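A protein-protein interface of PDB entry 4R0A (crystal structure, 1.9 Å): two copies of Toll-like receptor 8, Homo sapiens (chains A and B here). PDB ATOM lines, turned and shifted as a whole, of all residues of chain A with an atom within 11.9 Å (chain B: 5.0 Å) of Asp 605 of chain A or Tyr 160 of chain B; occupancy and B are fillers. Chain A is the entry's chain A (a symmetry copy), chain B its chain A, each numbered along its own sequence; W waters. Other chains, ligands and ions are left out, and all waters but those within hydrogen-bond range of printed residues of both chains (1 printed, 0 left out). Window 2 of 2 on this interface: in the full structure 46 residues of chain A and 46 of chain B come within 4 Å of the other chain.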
ATOM      1  N   TYR A 575      25.142 -20.043  11.713  1.00  0.00           N
ATOM      2  CA  TYR A 575      25.260 -18.597  11.799  1.00  0.00           C
ATOM      3  C   TYR A 575      25.204 -18.101  13.188  1.00  0.00           C
ATOM      4  O   TYR A 575      25.333 -16.907  13.402  1.00  0.00           O
ATOM      5  CB  TYR A 575      24.169 -17.884  10.944  1.00  0.00           C
ATOM      6  CG  TYR A 575      22.752 -17.999  11.438  1.00  0.00           C
ATOM      7  CD1 TYR A 575      21.998 -19.140  11.205  1.00  0.00           C
ATOM      8  CD2 TYR A 575      22.137 -16.933  12.127  1.00  0.00           C
ATOM      9  CE1 TYR A 575      20.684 -19.237  11.637  1.00  0.00           C
ATOM     10  CE2 TYR A 575      20.828 -17.017  12.550  1.00  0.00           C
ATOM     11  CZ  TYR A 575      20.099 -18.168  12.310  1.00  0.00           C
ATOM     12  OH  TYR A 575      18.777 -18.236  12.728  1.00  0.00           O
ATOM     13  N   TYR A 581      31.849 -19.319  21.294  1.00  0.00           N
ATOM     14  CA  TYR A 581      31.832 -18.882  19.928  1.00  0.00           C
ATOM     15  C   TYR A 581      33.023 -19.391  19.164  1.00  0.00           C
ATOM     16  O   TYR A 581      33.196 -19.063  17.968  1.00  0.00           O
ATOM     17  CB  TYR A 581      31.817 -17.350  19.913  1.00  0.00           C
ATOM     18  CG  TYR A 581      30.688 -16.786  20.788  1.00  0.00           C
ATOM     19  CD1 TYR A 581      29.383 -17.164  20.578  1.00  0.00           C
ATOM     20  CD2 TYR A 581      30.949 -15.889  21.827  1.00  0.00           C
ATOM     21  CE1 TYR A 581      28.350 -16.633  21.301  1.00  0.00           C
ATOM     22  CE2 TYR A 581      29.921 -15.349  22.586  1.00  0.00           C
ATOM     23  CZ  TYR A 581      28.620 -15.727  22.321  1.00  0.00           C
ATOM     24  OH  TYR A 581      27.567 -15.274  23.073  1.00  0.00           O
ATOM     25  N   LEU A 598      29.298 -17.689   7.267  1.00  0.00           N
ATOM     26  CA  LEU A 598      30.367 -16.900   7.816  1.00  0.00           C
ATOM     27  C   LEU A 598      30.112 -15.438   7.508  1.00  0.00           C
ATOM     28  O   LEU A 598      30.610 -14.534   8.237  1.00  0.00           O
ATOM     29  CB  LEU A 598      31.725 -17.328   7.288  1.00  0.00           C
ATOM     30  CG  LEU A 598      32.360 -18.515   8.029  1.00  0.00           C
ATOM     31  CD1 LEU A 598      33.477 -19.108   7.195  1.00  0.00           C
ATOM     32  CD2 LEU A 598      32.843 -18.165   9.416  1.00  0.00           C
ATOM     33  N   ASP A 599      29.321 -15.176   6.458  1.00  0.00           N
ATOM     34  CA  ASP A 599      28.923 -13.771   6.168  1.00  0.00           C
ATOM     35  C   ASP A 599      28.208 -13.109   7.348  1.00  0.00           C
ATOM     36  O   ASP A 599      28.478 -11.979   7.690  1.00  0.00           O
ATOM     37  CB  ASP A 599      28.076 -13.693   4.887  1.00  0.00           C
ATOM     38  CG  ASP A 599      26.702 -14.262   5.055  1.00  0.00           C
ATOM     39  OD1 ASP A 599      26.559 -15.365   5.650  1.00  0.00           O
ATOM     40  OD2 ASP A 599      25.746 -13.629   4.516  1.00  0.00           O
ATOM     41  N   ILE A 600      27.375 -13.857   8.052  1.00  0.00           N
ATOM     42  CA  ILE A 600      26.759 -13.401   9.266  1.00  0.00           C
ATOM     43  C   ILE A 600      27.664 -13.536  10.496  1.00  0.00           C
ATOM     44  O   ILE A 600      27.727 -12.637  11.363  1.00  0.00           O
ATOM     45  CB  ILE A 600      25.475 -14.198   9.491  1.00  0.00           C
ATOM     46  CG1 ILE A 600      24.418 -13.816   8.449  1.00  0.00           C
ATOM     47  CG2 ILE A 600      24.931 -14.018  10.898  1.00  0.00           C
ATOM     48  CD1 ILE A 600      23.156 -14.674   8.593  1.00  0.00           C
ATOM     49  N   LEU A 601      28.344 -14.668  10.638  1.00  0.00           N
ATOM     50  CA  LEU A 601      29.239 -14.829  11.825  1.00  0.00           C
ATOM     51  C   LEU A 601      30.297 -13.681  11.945  1.00  0.00           C
ATOM     52  O   LEU A 601      30.585 -13.212  13.045  1.00  0.00           O
ATOM     53  CB  LEU A 601      29.958 -16.189  11.777  1.00  0.00           C
ATOM     54  CG  LEU A 601      29.021 -17.375  11.847  1.00  0.00           C
ATOM     55  CD1 LEU A 601      29.678 -18.638  11.275  1.00  0.00           C
ATOM     56  CD2 LEU A 601      28.576 -17.531  13.279  1.00  0.00           C
ATOM     57  N   TRP A 602      30.866 -13.275  10.796  1.00  0.00           N
ATOM     58  CA  TRP A 602      31.892 -12.240  10.714  1.00  0.00           C
ATOM     59  C   TRP A 602      31.331 -10.860  10.301  1.00  0.00           C
ATOM     60  O   TRP A 602      32.073 -10.020   9.752  1.00  0.00           O
ATOM     61  CB  TRP A 602      32.971 -12.619   9.714  1.00  0.00           C
ATOM     62  CG  TRP A 602      33.856 -13.750  10.189  1.00  0.00           C
ATOM     63  CD1 TRP A 602      34.075 -14.125  11.471  1.00  0.00           C
ATOM     64  CD2 TRP A 602      34.667 -14.601   9.383  1.00  0.00           C
ATOM     65  NE1 TRP A 602      34.988 -15.157  11.522  1.00  0.00           N
ATOM     66  CE2 TRP A 602      35.371 -15.462  10.257  1.00  0.00           C
ATOM     67  CE3 TRP A 602      34.880 -14.714   8.010  1.00  0.00           C
ATOM     68  CZ2 TRP A 602      36.228 -16.443   9.799  1.00  0.00           C
ATOM     69  CZ3 TRP A 602      35.739 -15.674   7.559  1.00  0.00           C
ATOM     70  CH2 TRP A 602      36.403 -16.527   8.452  1.00  0.00           C
ATOM     71  N   ASN A 603      30.037 -10.653  10.554  1.00  0.00           N
ATOM     72  CA  ASN A 603      29.392  -9.355  10.307  1.00  0.00           C
ATOM     73  C   ASN A 603      30.194  -8.201  10.988  1.00  0.00           C
ATOM     74  O   ASN A 603      30.547  -8.282  12.151  1.00  0.00           O
ATOM     75  CB  ASN A 603      27.956  -9.422  10.855  1.00  0.00           C
ATOM     76  CG  ASN A 603      27.283  -8.100  10.823  1.00  0.00           C
ATOM     77  OD1 ASN A 603      27.335  -7.330  11.804  1.00  0.00           O
ATOM     78  ND2 ASN A 603      26.695  -7.776   9.673  1.00  0.00           N
ATOM     79  N   ASP A 604      30.490  -7.139  10.254  1.00  0.00           N
ATOM     80  CA  ASP A 604      31.237  -6.004  10.842  1.00  0.00           C
ATOM     81  C   ASP A 604      30.765  -5.521  12.230  1.00  0.00           C
ATOM     82  O   ASP A 604      31.553  -5.028  12.997  1.00  0.00           O
ATOM     83  CB  ASP A 604      31.193  -4.819   9.883  1.00  0.00           C
ATOM     84  CG  ASP A 604      31.903  -5.104   8.573  1.00  0.00           C
ATOM     85  OD1 ASP A 604      32.912  -5.846   8.585  1.00  0.00           O
ATOM     86  OD2 ASP A 604      31.426  -4.607   7.527  1.00  0.00           O
ATOM     87  N   ASP A 605      29.478  -5.594  12.556  1.00  0.00           N
ATOM     88  CA  ASP A 605      29.045  -5.109  13.851  1.00  0.00           C
ATOM     89  C   ASP A 605      29.157  -6.145  14.980  1.00  0.00           C
ATOM     90  O   ASP A 605      28.647  -5.921  16.100  1.00  0.00           O
ATOM     91  CB  ASP A 605      27.586  -4.642  13.772  1.00  0.00           C
ATOM     92  CG  ASP A 605      27.363  -3.529  12.733  1.00  0.00           C
ATOM     93  OD1 ASP A 605      28.147  -2.583  12.661  1.00  0.00           O
ATOM     94  OD2 ASP A 605      26.388  -3.626  11.968  1.00  0.00           O
ATOM     95  N   ASP A 606      29.786  -7.291  14.715  1.00  0.00           N
ATOM     96  CA  ASP A 606      29.793  -8.390  15.717  1.00  0.00           C
ATOM     97  C   ASP A 606      31.204  -8.911  15.815  1.00  0.00           C
ATOM     98  O   ASP A 606      31.765  -9.405  14.840  1.00  0.00           O
ATOM     99  CB  ASP A 606      28.899  -9.540  15.281  1.00  0.00           C
ATOM    100  CG  ASP A 606      28.802 -10.665  16.333  1.00  0.00           C
ATOM    101  OD1 ASP A 606      29.356 -10.565  17.443  1.00  0.00           O
ATOM    102  OD2 ASP A 606      27.942 -11.535  16.128  1.00  0.00           O
ATOM    103  N   ASN A 607      31.749  -8.859  17.009  1.00  0.00           N
ATOM    104  CA  ASN A 607      33.109  -9.301  17.229  1.00  0.00           C
ATOM    105  C   ASN A 607      33.247 -10.714  17.782  1.00  0.00           C
ATOM    106  O   ASN A 607      34.341 -11.212  17.952  1.00  0.00           O
ATOM    107  CB  ASN A 607      33.764  -8.304  18.192  1.00  0.00           C
ATOM    108  CG  ASN A 607      34.054  -6.989  17.514  1.00  0.00           C
ATOM    109  OD1 ASN A 607      34.221  -6.933  16.278  1.00  0.00           O
ATOM    110  ND2 ASN A 607      34.107  -5.921  18.301  1.00  0.00           N
ATOM    111  N   ARG A 608      32.150 -11.318  18.169  1.00  0.00           N
ATOM    112  CA  ARG A 608      32.230 -12.530  18.918  1.00  0.00           C
ATOM    113  C   ARG A 608      32.886 -13.710  18.141  1.00  0.00           C
ATOM    114  O   ARG A 608      33.422 -14.591  18.767  1.00  0.00           O
ATOM    115  CB  ARG A 608      30.827 -12.930  19.355  1.00  0.00           C
ATOM    116  CG  ARG A 608      30.205 -12.047  20.433  1.00  0.00           C
ATOM    117  CD  ARG A 608      28.732 -12.367  20.661  1.00  0.00           C
ATOM    118  NE  ARG A 608      27.980 -12.238  19.392  1.00  0.00           N
ATOM    119  CZ  ARG A 608      26.811 -12.835  19.129  1.00  0.00           C
ATOM    120  NH1 ARG A 608      26.237 -13.675  20.018  1.00  0.00           N
ATOM    121  NH2 ARG A 608      26.274 -12.684  17.935  1.00  0.00           N
ATOM    122  N   TYR A 609      32.824 -13.746  16.804  1.00  0.00           N
ATOM    123  CA  TYR A 609      33.321 -14.936  16.078  1.00  0.00           C
ATOM    124  C   TYR A 609      34.671 -14.662  15.348  1.00  0.00           C
ATOM    125  O   TYR A 609      35.124 -15.432  14.504  1.00  0.00           O
ATOM    126  CB  TYR A 609      32.256 -15.478  15.108  1.00  0.00           C
ATOM    127  CG  TYR A 609      30.958 -15.913  15.774  1.00  0.00           C
ATOM    128  CD1 TYR A 609      30.826 -17.155  16.384  1.00  0.00           C
ATOM    129  CD2 TYR A 609      29.849 -15.034  15.822  1.00  0.00           C
ATOM    130  CE1 TYR A 609      29.617 -17.524  17.046  1.00  0.00           C
ATOM    131  CE2 TYR A 609      28.650 -15.426  16.384  1.00  0.00           C
ATOM    132  CZ  TYR A 609      28.532 -16.639  16.991  1.00  0.00           C
ATOM    133  OH  TYR A 609      27.318 -16.921  17.574  1.00  0.00           O
ATOM    134  N   ILE A 610      35.323 -13.578  15.725  1.00  0.00           N
ATOM    135  CA  ILE A 610      36.495 -13.106  15.022  1.00  0.00           C
ATOM    136  C   ILE A 610      37.701 -14.066  15.178  1.00  0.00           C
ATOM    137  O   ILE A 610      38.580 -14.047  14.355  1.00  0.00           O
ATOM    138  CB  ILE A 610      36.910 -11.728  15.561  1.00  0.00           C
ATOM    139  CG1 ILE A 610      37.480 -10.895  14.454  1.00  0.00           C
ATOM    140  CG2 ILE A 610      37.882 -11.847  16.718  1.00  0.00           C
ATOM    141  CD1 ILE A 610      36.350 -10.361  13.584  1.00  0.00           C
ATOM    142  N   HIS A 631      33.078  -9.941   1.833  1.00  0.00           N
ATOM    143  CA  HIS A 631      34.457  -9.651   2.241  1.00  0.00           C
ATOM    144  C   HIS A 631      34.782 -10.395   3.527  1.00  0.00           C
ATOM    145  O   HIS A 631      33.895 -10.858   4.248  1.00  0.00           O
ATOM    146  CB  HIS A 631      34.641  -8.154   2.464  1.00  0.00           C
ATOM    147  CG  HIS A 631      33.839  -7.635   3.603  1.00  0.00           C
ATOM    148  ND1 HIS A 631      32.475  -7.435   3.516  1.00  0.00           N
ATOM    149  CD2 HIS A 631      34.179  -7.367   4.887  1.00  0.00           C
ATOM    150  CE1 HIS A 631      32.015  -7.036   4.688  1.00  0.00           C
ATOM    151  NE2 HIS A 631      33.028  -6.987   5.537  1.00  0.00           N
ATOM    152  N   ILE A 632      36.061 -10.488   3.826  1.00  0.00           N
ATOM    153  CA  ILE A 632      36.482 -11.054   5.094  1.00  0.00           C
ATOM    154  C   ILE A 632      37.192  -9.966   5.884  1.00  0.00           C
ATOM    155  O   ILE A 632      38.125  -9.367   5.371  1.00  0.00           O
ATOM    156  CB  ILE A 632      37.438 -12.222   4.853  1.00  0.00           C
ATOM    157  CG1 ILE A 632      36.715 -13.320   4.060  1.00  0.00           C
ATOM    158  CG2 ILE A 632      37.928 -12.789   6.187  1.00  0.00           C
ATOM    159  CD1 ILE A 632      37.630 -14.408   3.554  1.00  0.00           C
ATOM    160  N   PRO A 633      36.722  -9.674   7.100  1.00  0.00           N
ATOM    161  CA  PRO A 633      37.390  -8.667   7.888  1.00  0.00           C
ATOM    162  C   PRO A 633      38.860  -9.075   8.110  1.00  0.00           C
ATOM    163  O   PRO A 633      39.182 -10.266   8.282  1.00  0.00           O
ATOM    164  CB  PRO A 633      36.606  -8.683   9.215  1.00  0.00           C
ATOM    165  CG  PRO A 633      35.282  -9.254   8.868  1.00  0.00           C
ATOM    166  CD  PRO A 633      35.597 -10.281   7.837  1.00  0.00           C
ATOM    167  N   ASN A 634      39.751  -8.108   7.975  1.00  0.00           N
ATOM    168  CA  ASN A 634      41.179  -8.397   8.022  1.00  0.00           C
ATOM    169  C   ASN A 634      41.515  -9.158   9.314  1.00  0.00           C
ATOM    170  O   ASN A 634      42.244 -10.123   9.263  1.00  0.00           O
ATOM    171  CB  ASN A 634      41.984  -7.124   7.916  1.00  0.00           C
ATOM    172  CG  ASN A 634      41.874  -6.488   6.546  1.00  0.00           C
ATOM    173  OD1 ASN A 634      42.024  -7.153   5.527  1.00  0.00           O
ATOM    174  ND2 ASN A 634      41.707  -5.178   6.517  1.00  0.00           N
ATOM    175  N   GLU A 635      40.924  -8.731  10.424  1.00  0.00           N
ATOM    176  CA  GLU A 635      41.157  -9.368  11.724  1.00  0.00           C
ATOM    177  C   GLU A 635      40.708 -10.833  11.714  1.00  0.00           C
ATOM    178  O   GLU A 635      41.353 -11.668  12.351  1.00  0.00           O
ATOM    179  CB  GLU A 635      40.490  -8.601  12.879  1.00  0.00           C
ATOM    180  CG  GLU A 635      40.705  -9.263  14.261  1.00  0.00           C
ATOM    181  CD  GLU A 635      40.296  -8.401  15.478  1.00  0.00           C
ATOM    182  OE1 GLU A 635      39.759  -7.288  15.274  1.00  0.00           O
ATOM    183  OE2 GLU A 635      40.504  -8.846  16.648  1.00  0.00           O
ATOM    184  N   ALA A 636      39.613 -11.133  11.013  1.00  0.00           N
ATOM    185  CA  ALA A 636      39.087 -12.500  10.960  1.00  0.00           C
ATOM    186  C   ALA A 636      40.033 -13.361  10.160  1.00  0.00           C
ATOM    187  O   ALA A 636      40.317 -14.469  10.550  1.00  0.00           O
ATOM    188  CB  ALA A 636      37.669 -12.522  10.350  1.00  0.00           C
ATOM    189  N   GLN B 133      20.589   4.241  10.209  1.00  0.00           N
ATOM    190  CA  GLN B 133      21.891   3.656   9.754  1.00  0.00           C
ATOM    191  C   GLN B 133      22.938   4.653   9.265  1.00  0.00           C
ATOM    192  O   GLN B 133      23.455   4.525   8.180  1.00  0.00           O
ATOM    193  CB  GLN B 133      21.646   2.625   8.640  1.00  0.00           C
ATOM    194  CG  GLN B 133      21.343   1.245   9.162  1.00  0.00           C
ATOM    195  CD  GLN B 133      22.538   0.653   9.871  1.00  0.00           C
ATOM    196  OE1 GLN B 133      23.607   1.187   9.775  1.00  0.00           O
ATOM    197  NE2 GLN B 133      22.368  -0.502  10.504  1.00  0.00           N
ATOM    198  N   TRP B 157      19.266   2.965  14.669  1.00  0.00           N
ATOM    199  CA  TRP B 157      20.444   2.210  14.170  1.00  0.00           C
ATOM    200  C   TRP B 157      21.624   3.116  13.815  1.00  0.00           C
ATOM    201  O   TRP B 157      22.319   2.873  12.837  1.00  0.00           O
ATOM    202  CB  TRP B 157      20.083   1.336  12.941  1.00  0.00           C
ATOM    203  CG  TRP B 157      19.109   0.203  13.221  1.00  0.00           C
ATOM    204  CD1 TRP B 157      17.727   0.229  13.074  1.00  0.00           C
ATOM    205  CD2 TRP B 157      19.431  -1.119  13.649  1.00  0.00           C
ATOM    206  NE1 TRP B 157      17.207  -0.980  13.424  1.00  0.00           N
ATOM    207  CE2 TRP B 157      18.224  -1.822  13.782  1.00  0.00           C
ATOM    208  CE3 TRP B 157      20.632  -1.768  13.972  1.00  0.00           C
ATOM    209  CZ2 TRP B 157      18.176  -3.159  14.166  1.00  0.00           C
ATOM    210  CZ3 TRP B 157      20.581  -3.099  14.355  1.00  0.00           C
ATOM    211  CH2 TRP B 157      19.360  -3.779  14.440  1.00  0.00           C
ATOM    212  N   ASN B 158      21.948   4.074  14.678  1.00  0.00           N
ATOM    213  CA  ASN B 158      23.209   4.819  14.477  1.00  0.00           C
ATOM    214  C   ASN B 158      24.322   4.295  15.425  1.00  0.00           C
ATOM    215  O   ASN B 158      25.507   4.519  15.168  1.00  0.00           O
ATOM    216  CB  ASN B 158      22.997   6.354  14.595  1.00  0.00           C
ATOM    217  CG  ASN B 158      22.442   6.985  13.333  1.00  0.00           C
ATOM    218  OD1 ASN B 158      23.094   7.810  12.682  1.00  0.00           O
ATOM    219  ND2 ASN B 158      21.256   6.554  12.924  1.00  0.00           N
ATOM    220  N   CYS B 159      23.968   3.536  16.462  1.00  0.00           N
ATOM    221  CA  CYS B 159      24.986   3.046  17.437  1.00  0.00           C
ATOM    222  C   CYS B 159      24.520   1.823  18.191  1.00  0.00           C
ATOM    223  O   CYS B 159      23.632   1.918  19.032  1.00  0.00           O
ATOM    224  CB  CYS B 159      25.314   4.103  18.484  1.00  0.00           C
ATOM    225  SG  CYS B 159      26.684   3.665  19.600  1.00  0.00           S
ATOM    226  N   TYR B 160      25.108   0.661  17.901  1.00  0.00           N
ATOM    227  CA  TYR B 160      24.520  -0.575  18.402  1.00  0.00           C
ATOM    228  C   TYR B 160      25.555  -1.681  18.319  1.00  0.00           C
ATOM    229  O   TYR B 160      26.568  -1.531  17.631  1.00  0.00           O
ATOM    230  CB  TYR B 160      23.277  -0.941  17.533  1.00  0.00           C
ATOM    231  CG  TYR B 160      23.591  -1.015  16.045  1.00  0.00           C
ATOM    232  CD1 TYR B 160      23.651   0.125  15.241  1.00  0.00           C
ATOM    233  CD2 TYR B 160      23.949  -2.235  15.469  1.00  0.00           C
ATOM    234  CE1 TYR B 160      24.027   0.041  13.899  1.00  0.00           C
ATOM    235  CE2 TYR B 160      24.304  -2.349  14.138  1.00  0.00           C
ATOM    236  CZ  TYR B 160      24.376  -1.226  13.360  1.00  0.00           C
ATOM    237  OH  TYR B 160      24.766  -1.375  12.080  1.00  0.00           O
ATOM    238  N   PHE B 161      25.281  -2.776  19.028  1.00  0.00           N
ATOM    239  CA  PHE B 161      26.097  -3.992  18.962  1.00  0.00           C
ATOM    240  C   PHE B 161      27.553  -3.593  19.240  1.00  0.00           C
ATOM    241  O   PHE B 161      27.782  -2.884  20.200  1.00  0.00           O
ATOM    242  CB  PHE B 161      25.929  -4.708  17.612  1.00  0.00           C
ATOM    243  CG  PHE B 161      24.519  -5.161  17.300  1.00  0.00           C
ATOM    244  CD1 PHE B 161      23.517  -5.207  18.283  1.00  0.00           C
ATOM    245  CD2 PHE B 161      24.226  -5.644  16.048  1.00  0.00           C
ATOM    246  CE1 PHE B 161      22.236  -5.640  17.974  1.00  0.00           C
ATOM    247  CE2 PHE B 161      22.928  -6.071  15.736  1.00  0.00           C
ATOM    248  CZ  PHE B 161      21.956  -6.090  16.702  1.00  0.00           C
ATOM    249  N   ASN B 162      28.514  -3.997  18.398  1.00  0.00           N
ATOM    250  CA  ASN B 162      29.925  -3.703  18.615  1.00  0.00           C
ATOM    251  C   ASN B 162      30.431  -2.733  17.594  1.00  0.00           C
ATOM    252  O   ASN B 162      31.635  -2.617  17.386  1.00  0.00           O
ATOM    253  CB  ASN B 162      30.789  -4.960  18.513  1.00  0.00           C
ATOM    254  CG  ASN B 162      30.486  -5.979  19.605  1.00  0.00           C
ATOM    255  OD1 ASN B 162      30.544  -7.204  19.371  1.00  0.00           O
ATOM    256  ND2 ASN B 162      30.121  -5.497  20.780  1.00  0.00           N
ATOM    257  N   LYS B 163      29.529  -1.948  17.015  1.00  0.00           N
ATOM    258  CA  LYS B 163      29.926  -0.810  16.220  1.00  0.00           C
ATOM    259  C   LYS B 163      30.741   0.114  17.057  1.00  0.00           C
ATOM    260  O   LYS B 163      30.430   0.320  18.228  1.00  0.00           O
ATOM    261  CB  LYS B 163      28.680  -0.036  15.764  1.00  0.00           C
ATOM    262  CG  LYS B 163      29.002   1.003  14.727  1.00  0.00           C
ATOM    263  CD  LYS B 163      27.777   1.807  14.358  1.00  0.00           C
ATOM    264  CE  LYS B 163      28.194   2.782  13.279  1.00  0.00           C
ATOM    265  NZ  LYS B 163      27.062   3.718  13.075  1.00  0.00           N
ATOM    266  N   CYS B 165      31.229   3.602  18.112  1.00  0.00           N
ATOM    267  CA  CYS B 165      30.329   4.762  18.099  1.00  0.00           C
ATOM    268  C   CYS B 165      30.176   5.375  19.485  1.00  0.00           C
ATOM    269  O   CYS B 165      30.386   4.704  20.512  1.00  0.00           O
ATOM    270  CB  CYS B 165      28.942   4.348  17.523  1.00  0.00           C
ATOM    271  SG  CYS B 165      28.150   2.942  18.339  1.00  0.00           S
ATOM    272  N   PHE B 188      18.085   1.341  18.727  1.00  0.00           N
ATOM    273  CA  PHE B 188      19.451   0.955  18.288  1.00  0.00           C
ATOM    274  C   PHE B 188      20.388   2.153  18.234  1.00  0.00           C
ATOM    275  O   PHE B 188      21.108   2.385  17.290  1.00  0.00           O
ATOM    276  CB  PHE B 188      19.457   0.083  16.985  1.00  0.00           C
ATOM    277  CG  PHE B 188      18.677  -1.198  17.145  1.00  0.00           C
ATOM    278  CD1 PHE B 188      17.312  -1.234  16.877  1.00  0.00           C
ATOM    279  CD2 PHE B 188      19.267  -2.328  17.699  1.00  0.00           C
ATOM    280  CE1 PHE B 188      16.559  -2.380  17.137  1.00  0.00           C
ATOM    281  CE2 PHE B 188      18.528  -3.486  17.881  1.00  0.00           C
ATOM    282  CZ  PHE B 188      17.180  -3.518  17.610  1.00  0.00           C
ATOM    283  N   PRO B 244      25.492  -9.338  19.271  1.00  0.00           N
ATOM    284  CA  PRO B 244      26.185  -8.937  20.481  1.00  0.00           C
ATOM    285  C   PRO B 244      25.240  -8.307  21.513  1.00  0.00           C
ATOM    286  O   PRO B 244      24.546  -7.358  21.218  1.00  0.00           O
ATOM    287  CB  PRO B 244      27.223  -7.923  19.998  1.00  0.00           C
ATOM    288  CG  PRO B 244      27.309  -8.067  18.538  1.00  0.00           C
ATOM    289  CD  PRO B 244      26.040  -8.693  18.062  1.00  0.00           C
HETATM  290  O   HOH W   1      27.822  -0.555  11.246  1.00  0.00           O
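Water W1 bridges the side-chain carboxylate of Asp 605 of chain A (2.5 Å) and the side-chain hydroxyl of Tyr 160 of chain B (3.3 Å).
Among the printed residues, merely in contact across the chains: Asp 605 of chain A with Phe 161 of chain B (3.3 Å), Asp 605 of chain A with Pro 244 of chain B (3.5 Å), Asp 606 of chain A with Asn 162 of chain B (3.9 Å), Asp 606 of chain A with Pro 244 of chain B (3.4 Å) and Arg 608 of chain A with Pro 244 of chain B (3.7 Å).
The side-chain carboxylate (OD2) of Asp 606 of chain A lies within salt-bridge range of the guanidinium group (NH2) of Arg 608 of chain A.
OH of Tyr 160 of chain B lies within hydrogen-bond range of NE2 of Gln 133 of chain B (3.0 Å).
SG of Cys 159 of chain B is disulfide-bonded to SG of Cys 165 of chain B (2.1 Å).
OD1 of Asn 603 of chain A lies within hydrogen-bond range of N of Asp 605 of chain A.
No position is printed for both chains.
Of the 21 printed residues of chain A, 4 touch a printed residue of chain B.
Hydrophobic or aromatic side chains of chain B that line the printed part of chain A: Tyr 160, Phe 161 and Pro 244.
Among the printed residues, 8 pairs touch across the chains.
Leu 598 of chain A touches none of the printed residues of chain B.
Asp 605 of chain A touches four residues of chain B.
Of the printed residues of chain B, Asn 607 of chain A touches Asn 162.
Printed residues of chain B within 4 Å of Arg 608 of chain A: Pro 244 (3.7 Å).
Ile 632 of chain A touches none of the printed residues of chain B.
No residue of chain A comes within 4 Å of Gln 133 of chain B.
No residue of chain A comes within 4 Å of Cys 159 of chain B.
Printed residues of chain A within 4 Å of Tyr 160 of chain B: Asp 605.
Phe 161 of chain B touches just one residue of chain A: Asp 605.
No residue of chain A comes within 4 Å of Cys 165 of chain B.
No residue of chain A comes within 4 Å of Phe 188 of chain B.
Pro 244 of chain B touches three residues of chain A.
The nearest residue of chain A that does not touch Tyr 160 of chain B is Asn 603 of chain A (6.3 Å).
The nearest printed residue of chain B that does not touch Asp 606 of chain A is Phe 161 of chain B (5.5 Å).
The backbone carbonyl oxygen (O) of Asp 605 of chain A sits at hydrogen-bond distance from the backbone NH (N) of Asn 162 of chain B (3.0 Å).
The side-chain hydroxyl (OH) of Tyr 160 of chain B is in hydrogen-bond range of the side-chain carboxylate (OD2) of Asp 605 of chain A (2.8 Å).
OD1 of Asn 162 of chain B is in hydrogen-bond range of N of Asn 607 of chain A.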
